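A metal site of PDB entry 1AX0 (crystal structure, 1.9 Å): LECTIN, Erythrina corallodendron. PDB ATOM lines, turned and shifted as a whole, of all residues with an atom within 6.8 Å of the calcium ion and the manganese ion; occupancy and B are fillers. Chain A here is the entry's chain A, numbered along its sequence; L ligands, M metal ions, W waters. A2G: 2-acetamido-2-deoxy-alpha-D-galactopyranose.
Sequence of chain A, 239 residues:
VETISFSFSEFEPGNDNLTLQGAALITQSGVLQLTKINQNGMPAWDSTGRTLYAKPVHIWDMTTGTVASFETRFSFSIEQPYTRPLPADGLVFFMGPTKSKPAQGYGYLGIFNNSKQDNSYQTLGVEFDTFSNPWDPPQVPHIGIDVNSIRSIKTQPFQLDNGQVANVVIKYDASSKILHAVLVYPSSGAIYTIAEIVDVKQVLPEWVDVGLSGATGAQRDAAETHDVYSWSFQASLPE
The side-chain amide nitrogen (ND2) of Asn 133 is in hydrogen-bond range of an oxygen (O3) of the ligand, 2.9 Å away. An oxygen (O3) of the ligand lies within hydrogen-bond range of the backbone NH (N) of Gly 107. An oxygen (O3) of the ligand is in hydrogen-bond range of the side-chain carboxylate (OD1) of Asp 89, 2.7 Å away.
The side-chain carboxylate of Glu 127 sits close to the side-chain carboxylate of Asp 146, at 2.7 Å. The backbone NH (N) of Glu 127 is in hydrogen-bond range of the backbone carbonyl oxygen (O) of Gly 144, 2.9 Å away.
Four residues have an atom within 4 Å of the calcium ion: Asp 129, Phe 131, Asn 133 and Asp 136.
Within 4 Å of the manganese ion: Glu 127, Asp 129, Asp 136 and His 142.
The calcium ion is bound by O of Phe 131 (2.4 Å). The calcium ion is bound by OD1 of Asn 133, 2.4 Å away. The side-chain carboxylate (OD2) of Asp 129 is bound to the calcium ion (2.4 Å). The side-chain carboxylate (OD2) of Asp 136 is bound to the calcium ion (2.4 Å). Water W1 binds the calcium ion. Water W3 is bound to the calcium ion. The side-chain carboxylate (OD1) of Asp 129 is bound to the calcium ion.
The manganese ion is bound by OD2 of Asp 129 (2.4 Å), OD1 of Asp 136 (2.4 Å), OE2 of Glu 127 (2.4 Å), NE2 of His 142 (2.4 Å), water W4 (2.4 Å) and water W2 (2.5 Å). The manganese ion has six donor atoms within binding distance.
Water W3 lies within hydrogen-bond range of the backbone carbonyl oxygen of Gly 107 (2.7 Å) and the indole nitrogen of Trp 135 (3.1 Å). Water W2 lies within hydrogen-bond range of O of Ile 150, OE1 of Glu 127 and NE1 of Trp 135.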
ATOM      1  N   ASP A  89      25.233 -11.520  30.668  1.00  0.00           N
ATOM      2  CA  ASP A  89      25.026 -10.111  30.327  1.00  0.00           C
ATOM      3  C   ASP A  89      25.122  -9.200  31.559  1.00  0.00           C
ATOM      4  O   ASP A  89      25.408  -8.006  31.434  1.00  0.00           O
ATOM      5  CB  ASP A  89      23.649  -9.911  29.690  1.00  0.00           C
ATOM      6  CG  ASP A  89      23.677 -10.019  28.184  1.00  0.00           C
ATOM      7  OD1 ASP A  89      24.150  -9.068  27.519  1.00  0.00           O
ATOM      8  OD2 ASP A  89      23.241 -11.068  27.664  1.00  0.00           O
ATOM      9  N   TYR A 106      18.877 -11.269  28.052  1.00  0.00           N
ATOM     10  CA  TYR A 106      20.108 -10.803  27.398  1.00  0.00           C
ATOM     11  C   TYR A 106      20.497  -9.409  27.887  1.00  0.00           C
ATOM     12  O   TYR A 106      20.436  -9.134  29.098  1.00  0.00           O
ATOM     13  CB  TYR A 106      19.945 -10.812  25.869  1.00  0.00           C
ATOM     14  CG  TYR A 106      19.325 -12.083  25.332  1.00  0.00           C
ATOM     15  CD1 TYR A 106      19.729 -13.335  25.795  1.00  0.00           C
ATOM     16  CD2 TYR A 106      18.315 -12.032  24.379  1.00  0.00           C
ATOM     17  CE1 TYR A 106      19.137 -14.503  25.328  1.00  0.00           C
ATOM     18  CE2 TYR A 106      17.715 -13.198  23.901  1.00  0.00           C
ATOM     19  CZ  TYR A 106      18.122 -14.426  24.384  1.00  0.00           C
ATOM     20  OH  TYR A 106      17.531 -15.575  23.930  1.00  0.00           O
ATOM     21  N   GLY A 107      20.862  -8.526  26.966  1.00  0.00           N
ATOM     22  CA  GLY A 107      21.269  -7.173  27.323  1.00  0.00           C
ATOM     23  C   GLY A 107      20.213  -6.337  28.025  1.00  0.00           C
ATOM     24  O   GLY A 107      20.541  -5.296  28.591  1.00  0.00           O
ATOM     25  N   TYR A 108      18.959  -6.772  27.976  1.00  0.00           N
ATOM     26  CA  TYR A 108      17.868  -6.048  28.629  1.00  0.00           C
ATOM     27  C   TYR A 108      17.755  -6.410  30.100  1.00  0.00           C
ATOM     28  O   TYR A 108      16.943  -5.841  30.831  1.00  0.00           O
ATOM     29  CB  TYR A 108      16.554  -6.263  27.888  1.00  0.00           C
ATOM     30  CG  TYR A 108      16.654  -5.835  26.440  1.00  0.00           C
ATOM     31  CD1 TYR A 108      16.852  -4.502  26.112  1.00  0.00           C
ATOM     32  CD2 TYR A 108      16.598  -6.774  25.417  1.00  0.00           C
ATOM     33  CE1 TYR A 108      17.007  -4.109  24.795  1.00  0.00           C
ATOM     34  CE2 TYR A 108      16.747  -6.392  24.085  1.00  0.00           C
ATOM     35  CZ  TYR A 108      16.957  -5.055  23.775  1.00  0.00           C
ATOM     36  OH  TYR A 108      17.107  -4.661  22.472  1.00  0.00           O
ATOM     37  N   LEU A 109      18.556  -7.393  30.505  1.00  0.00           N
ATOM     38  CA  LEU A 109      18.652  -7.860  31.893  1.00  0.00           C
ATOM     39  C   LEU A 109      17.378  -8.322  32.599  1.00  0.00           C
ATOM     40  O   LEU A 109      17.345  -8.399  33.828  1.00  0.00           O
ATOM     41  CB  LEU A 109      19.339  -6.772  32.724  1.00  0.00           C
ATOM     42  CG  LEU A 109      20.684  -6.258  32.172  1.00  0.00           C
ATOM     43  CD1 LEU A 109      21.173  -5.079  33.003  1.00  0.00           C
ATOM     44  CD2 LEU A 109      21.709  -7.382  32.155  1.00  0.00           C
ATOM     45  N   GLU A 127      22.502  -1.299  37.563  1.00  0.00           N
ATOM     46  CA  GLU A 127      23.049  -2.467  36.904  1.00  0.00           C
ATOM     47  C   GLU A 127      24.542  -2.664  37.058  1.00  0.00           C
ATOM     48  O   GLU A 127      25.295  -1.729  37.307  1.00  0.00           O
ATOM     49  CB  GLU A 127      22.742  -2.382  35.416  1.00  0.00           C
ATOM     50  CG  GLU A 127      23.337  -1.121  34.807  1.00  0.00           C
ATOM     51  CD  GLU A 127      23.331  -1.128  33.320  1.00  0.00           C
ATOM     52  OE1 GLU A 127      22.278  -1.321  32.707  1.00  0.00           O
ATOM     53  OE2 GLU A 127      24.430  -0.925  32.772  1.00  0.00           O
ATOM     54  N   ASP A 129      26.703  -4.390  34.588  1.00  0.00           N
ATOM     55  CA  ASP A 129      26.726  -4.842  33.208  1.00  0.00           C
ATOM     56  C   ASP A 129      28.072  -5.395  32.735  1.00  0.00           C
ATOM     57  O   ASP A 129      29.065  -4.689  32.733  1.00  0.00           O
ATOM     58  CB  ASP A 129      26.327  -3.656  32.355  1.00  0.00           C
ATOM     59  CG  ASP A 129      25.891  -4.040  30.975  1.00  0.00           C
ATOM     60  OD1 ASP A 129      26.226  -5.136  30.487  1.00  0.00           O
ATOM     61  OD2 ASP A 129      25.195  -3.218  30.374  1.00  0.00           O
ATOM     62  N   THR A 130      28.038  -6.621  32.211  1.00  0.00           N
ATOM     63  CA  THR A 130      29.244  -7.304  31.767  1.00  0.00           C
ATOM     64  C   THR A 130      29.458  -7.410  30.251  1.00  0.00           C
ATOM     65  O   THR A 130      30.513  -7.878  29.805  1.00  0.00           O
ATOM     66  CB  THR A 130      29.299  -8.716  32.373  1.00  0.00           C
ATOM     67  OG1 THR A 130      28.119  -9.440  32.000  1.00  0.00           O
ATOM     68  CG2 THR A 130      29.382  -8.641  33.886  1.00  0.00           C
ATOM     69  N   PHE A 131      28.490  -6.972  29.460  1.00  0.00           N
ATOM     70  CA  PHE A 131      28.619  -7.048  28.007  1.00  0.00           C
ATOM     71  C   PHE A 131      28.282  -5.704  27.364  1.00  0.00           C
ATOM     72  O   PHE A 131      27.264  -5.119  27.677  1.00  0.00           O
ATOM     73  CB  PHE A 131      27.697  -8.144  27.449  1.00  0.00           C
ATOM     74  CG  PHE A 131      27.785  -8.306  25.958  1.00  0.00           C
ATOM     75  CD1 PHE A 131      28.702  -9.184  25.402  1.00  0.00           C
ATOM     76  CD2 PHE A 131      26.955  -7.568  25.109  1.00  0.00           C
ATOM     77  CE1 PHE A 131      28.807  -9.317  24.012  1.00  0.00           C
ATOM     78  CE2 PHE A 131      27.050  -7.692  23.728  1.00  0.00           C
ATOM     79  CZ  PHE A 131      27.980  -8.574  23.170  1.00  0.00           C
ATOM     80  N   SER A 132      29.125  -5.257  26.437  1.00  0.00           N
ATOM     81  CA  SER A 132      28.887  -3.973  25.786  1.00  0.00           C
ATOM     82  C   SER A 132      27.960  -4.049  24.570  1.00  0.00           C
ATOM     83  O   SER A 132      28.371  -4.504  23.504  1.00  0.00           O
ATOM     84  CB  SER A 132      30.230  -3.332  25.388  1.00  0.00           C
ATOM     85  OG  SER A 132      30.033  -1.990  24.962  1.00  0.00           O
ATOM     86  N   ASN A 133      26.713  -3.629  24.766  1.00  0.00           N
ATOM     87  CA  ASN A 133      25.709  -3.597  23.696  1.00  0.00           C
ATOM     88  C   ASN A 133      25.883  -2.281  22.929  1.00  0.00           C
ATOM     89  O   ASN A 133      26.666  -1.428  23.338  1.00  0.00           O
ATOM     90  CB  ASN A 133      24.298  -3.696  24.291  1.00  0.00           C
ATOM     91  CG  ASN A 133      24.045  -5.010  24.984  1.00  0.00           C
ATOM     92  OD1 ASN A 133      24.194  -5.119  26.192  1.00  0.00           O
ATOM     93  ND2 ASN A 133      23.648  -6.026  24.223  1.00  0.00           N
ATOM     94  N   TRP A 135      24.147   0.315  22.893  1.00  0.00           N
ATOM     95  CA  TRP A 135      23.740   1.460  23.719  1.00  0.00           C
ATOM     96  C   TRP A 135      24.656   1.677  24.917  1.00  0.00           C
ATOM     97  O   TRP A 135      24.472   2.624  25.694  1.00  0.00           O
ATOM     98  CB  TRP A 135      22.302   1.250  24.223  1.00  0.00           C
ATOM     99  CG  TRP A 135      22.114  -0.038  24.988  1.00  0.00           C
ATOM    100  CD1 TRP A 135      22.502  -0.289  26.280  1.00  0.00           C
ATOM    101  CD2 TRP A 135      21.490  -1.233  24.514  1.00  0.00           C
ATOM    102  NE1 TRP A 135      22.151  -1.569  26.630  1.00  0.00           N
ATOM    103  CE2 TRP A 135      21.532  -2.180  25.567  1.00  0.00           C
ATOM    104  CE3 TRP A 135      20.913  -1.603  23.294  1.00  0.00           C
ATOM    105  CZ2 TRP A 135      21.004  -3.462  25.437  1.00  0.00           C
ATOM    106  CZ3 TRP A 135      20.383  -2.896  23.171  1.00  0.00           C
ATOM    107  CH2 TRP A 135      20.432  -3.803  24.244  1.00  0.00           C
ATOM    108  N   ASP A 136      25.641   0.790  25.070  1.00  0.00           N
ATOM    109  CA  ASP A 136      26.596   0.841  26.178  1.00  0.00           C
ATOM    110  C   ASP A 136      27.908   1.526  25.876  1.00  0.00           C
ATOM    111  O   ASP A 136      28.288   1.675  24.707  1.00  0.00           O
ATOM    112  CB  ASP A 136      26.986  -0.591  26.580  1.00  0.00           C
ATOM    113  CG  ASP A 136      25.914  -1.282  27.356  1.00  0.00           C
ATOM    114  OD1 ASP A 136      25.225  -0.598  28.113  1.00  0.00           O
ATOM    115  OD2 ASP A 136      25.740  -2.498  27.198  1.00  0.00           O
ATOM    116  N   PRO A 137      28.599   1.988  26.926  1.00  0.00           N
ATOM    117  CA  PRO A 137      29.890   2.629  26.714  1.00  0.00           C
ATOM    118  C   PRO A 137      30.781   1.425  26.396  1.00  0.00           C
ATOM    119  O   PRO A 137      30.429   0.277  26.717  1.00  0.00           O
ATOM    120  CB  PRO A 137      30.209   3.224  28.080  1.00  0.00           C
ATOM    121  CG  PRO A 137      29.490   2.318  29.038  1.00  0.00           C
ATOM    122  CD  PRO A 137      28.173   2.117  28.339  1.00  0.00           C
ATOM    123  N   VAL A 140      33.522  -2.451  29.892  1.00  0.00           N
ATOM    124  CA  VAL A 140      32.765  -3.425  30.656  1.00  0.00           C
ATOM    125  C   VAL A 140      33.758  -4.206  31.524  1.00  0.00           C
ATOM    126  O   VAL A 140      34.903  -4.416  31.131  1.00  0.00           O
ATOM    127  CB  VAL A 140      31.944  -4.419  29.785  1.00  0.00           C
ATOM    128  CG1 VAL A 140      30.729  -3.728  29.192  1.00  0.00           C
ATOM    129  CG2 VAL A 140      32.821  -5.018  28.680  1.00  0.00           C
ATOM    130  N   HIS A 142      30.621  -2.443  33.958  1.00  0.00           N
ATOM    131  CA  HIS A 142      30.364  -1.110  34.468  1.00  0.00           C
ATOM    132  C   HIS A 142      29.099  -1.081  35.300  1.00  0.00           C
ATOM    133  O   HIS A 142      28.224  -1.931  35.154  1.00  0.00           O
ATOM    134  CB  HIS A 142      30.293  -0.072  33.337  1.00  0.00           C
ATOM    135  CG  HIS A 142      29.257  -0.368  32.290  1.00  0.00           C
ATOM    136  ND1 HIS A 142      29.548  -0.902  31.057  1.00  0.00           N
ATOM    137  CD2 HIS A 142      27.912  -0.197  32.314  1.00  0.00           C
ATOM    138  CE1 HIS A 142      28.393  -1.035  30.390  1.00  0.00           C
ATOM    139  NE2 HIS A 142      27.374  -0.621  31.116  1.00  0.00           N
ATOM    140  N   ILE A 143      29.079  -0.152  36.245  1.00  0.00           N
ATOM    141  CA  ILE A 143      27.909   0.054  37.084  1.00  0.00           C
ATOM    142  C   ILE A 143      27.133   1.098  36.307  1.00  0.00           C
ATOM    143  O   ILE A 143      27.723   1.986  35.693  1.00  0.00           O
ATOM    144  CB  ILE A 143      28.276   0.682  38.448  1.00  0.00           C
ATOM    145  CG1 ILE A 143      29.334  -0.168  39.160  1.00  0.00           C
ATOM    146  CG2 ILE A 143      27.017   0.808  39.314  1.00  0.00           C
ATOM    147  CD1 ILE A 143      29.854   0.470  40.433  1.00  0.00           C
ATOM    148  N   GLY A 144      25.808   1.003  36.318  1.00  0.00           N
ATOM    149  CA  GLY A 144      25.026   1.991  35.607  1.00  0.00           C
ATOM    150  C   GLY A 144      23.728   2.286  36.319  1.00  0.00           C
ATOM    151  O   GLY A 144      23.166   1.421  36.970  1.00  0.00           O
ATOM    152  N   ASP A 146      20.013   3.197  35.710  1.00  0.00           N
ATOM    153  CA  ASP A 146      19.000   3.124  34.653  1.00  0.00           C
ATOM    154  C   ASP A 146      17.672   3.735  35.078  1.00  0.00           C
ATOM    155  O   ASP A 146      17.061   3.292  36.042  1.00  0.00           O
ATOM    156  CB  ASP A 146      18.763   1.651  34.275  1.00  0.00           C
ATOM    157  CG  ASP A 146      20.027   0.949  33.810  1.00  0.00           C
ATOM    158  OD1 ASP A 146      21.046   1.637  33.592  1.00  0.00           O
ATOM    159  OD2 ASP A 146      20.006  -0.284  33.655  1.00  0.00           O
ATOM    160  N   ILE A 150      17.403   1.084  29.429  1.00  0.00           N
ATOM    161  CA  ILE A 150      18.616   0.283  29.575  1.00  0.00           C
ATOM    162  C   ILE A 150      19.819   1.188  29.238  1.00  0.00           C
ATOM    163  O   ILE A 150      20.965   0.844  29.526  1.00  0.00           O
ATOM    164  CB  ILE A 150      18.559  -0.971  28.645  1.00  0.00           C
ATOM    165  CG1 ILE A 150      19.673  -1.956  28.995  1.00  0.00           C
ATOM    166  CG2 ILE A 150      18.572  -0.547  27.181  1.00  0.00           C
ATOM    167  CD1 ILE A 150      19.525  -2.577  30.379  1.00  0.00           C
ATOM    168  N   ARG A 151      19.542   2.334  28.609  1.00  0.00           N
ATOM    169  CA  ARG A 151      20.581   3.308  28.287  1.00  0.00           C
ATOM    170  C   ARG A 151      20.779   4.146  29.543  1.00  0.00           C
ATOM    171  O   ARG A 151      20.061   5.113  29.769  1.00  0.00           O
ATOM    172  CB  ARG A 151      20.156   4.224  27.146  1.00  0.00           C
ATOM    173  CG  ARG A 151      19.770   3.520  25.855  1.00  0.00           C
ATOM    174  CD  ARG A 151      19.700   4.533  24.728  1.00  0.00           C
ATOM    175  NE  ARG A 151      18.415   4.504  24.038  1.00  0.00           N
ATOM    176  CZ  ARG A 151      17.594   5.549  23.942  1.00  0.00           C
ATOM    177  NH1 ARG A 151      17.922   6.722  24.481  1.00  0.00           N
ATOM    178  NH2 ARG A 151      16.450   5.418  23.295  1.00  0.00           N
ATOM    179  N   SER A 152      21.794   3.785  30.340  1.00  0.00           N
ATOM    180  CA  SER A 152      22.075   4.453  31.606  1.00  0.00           C
ATOM    181  C   SER A 152      22.294   5.960  31.532  1.00  0.00           C
ATOM    182  O   SER A 152      22.889   6.463  30.583  1.00  0.00           O
ATOM    183  CB  SER A 152      23.301   3.828  32.276  1.00  0.00           C
ATOM    184  OG  SER A 152      23.184   2.417  32.335  1.00  0.00           O
ATOM    185  N   THR A 155      27.294   6.026  34.100  1.00  0.00           N
ATOM    186  CA  THR A 155      27.991   4.747  34.202  1.00  0.00           C
ATOM    187  C   THR A 155      29.364   4.916  34.850  1.00  0.00           C
ATOM    188  O   THR A 155      29.948   6.005  34.825  1.00  0.00           O
ATOM    189  CB  THR A 155      28.150   4.090  32.811  1.00  0.00           C
ATOM    190  OG1 THR A 155      28.673   2.758  32.965  1.00  0.00           O
ATOM    191  CG2 THR A 155      29.103   4.880  31.947  1.00  0.00           C
HETATM  192  O5  A2G L   1      24.335 -11.529  22.216  1.00  0.00           O
HETATM  193  C1  A2G L   1      23.588 -10.416  21.711  1.00  0.00           C
HETATM  194  O1  A2G L   1      24.481  -9.548  21.110  1.00  0.00           O
HETATM  195  C2  A2G L   1      22.861  -9.692  22.851  1.00  0.00           C
HETATM  196  N2  A2G L   1      22.230  -8.488  22.329  1.00  0.00           N
HETATM  197  C3  A2G L   1      23.833  -9.308  23.975  1.00  0.00           C
HETATM  198  O3  A2G L   1      23.109  -8.768  25.076  1.00  0.00           O
HETATM  199  C4  A2G L   1      24.623 -10.534  24.413  1.00  0.00           C
HETATM  200  O4  A2G L   1      23.735 -11.489  24.984  1.00  0.00           O
HETATM  201  C5  A2G L   1      25.323 -11.138  23.200  1.00  0.00           C
HETATM  202  C6  A2G L   1      26.125 -12.372  23.538  1.00  0.00           C
HETATM  203  O6  A2G L   1      26.973 -12.743  22.464  1.00  0.00           O
HETATM  204  C7  A2G L   1      20.929  -8.295  22.486  1.00  0.00           C
HETATM  205  O7  A2G L   1      20.192  -9.084  23.063  1.00  0.00           O
HETATM  206  C8  A2G L   1      20.353  -7.007  21.910  1.00  0.00           C
HETATM  207 CA    CA M   1      25.056  -4.518  28.344  1.00  0.00          CA
HETATM  208 MN    MN M   2      25.049  -0.861  30.472  1.00  0.00          MN
HETATM  209  O   HOH W   1      24.478  -6.813  28.925  1.00  0.00           O
HETATM  210  O   HOH W   2      22.642  -1.145  30.056  1.00  0.00           O
HETATM  211  O   HOH W   3      22.773  -3.777  28.788  1.00  0.00           O
HETATM  212  O   HOH W   4      24.938   1.573  30.503  1.00  0.00           O
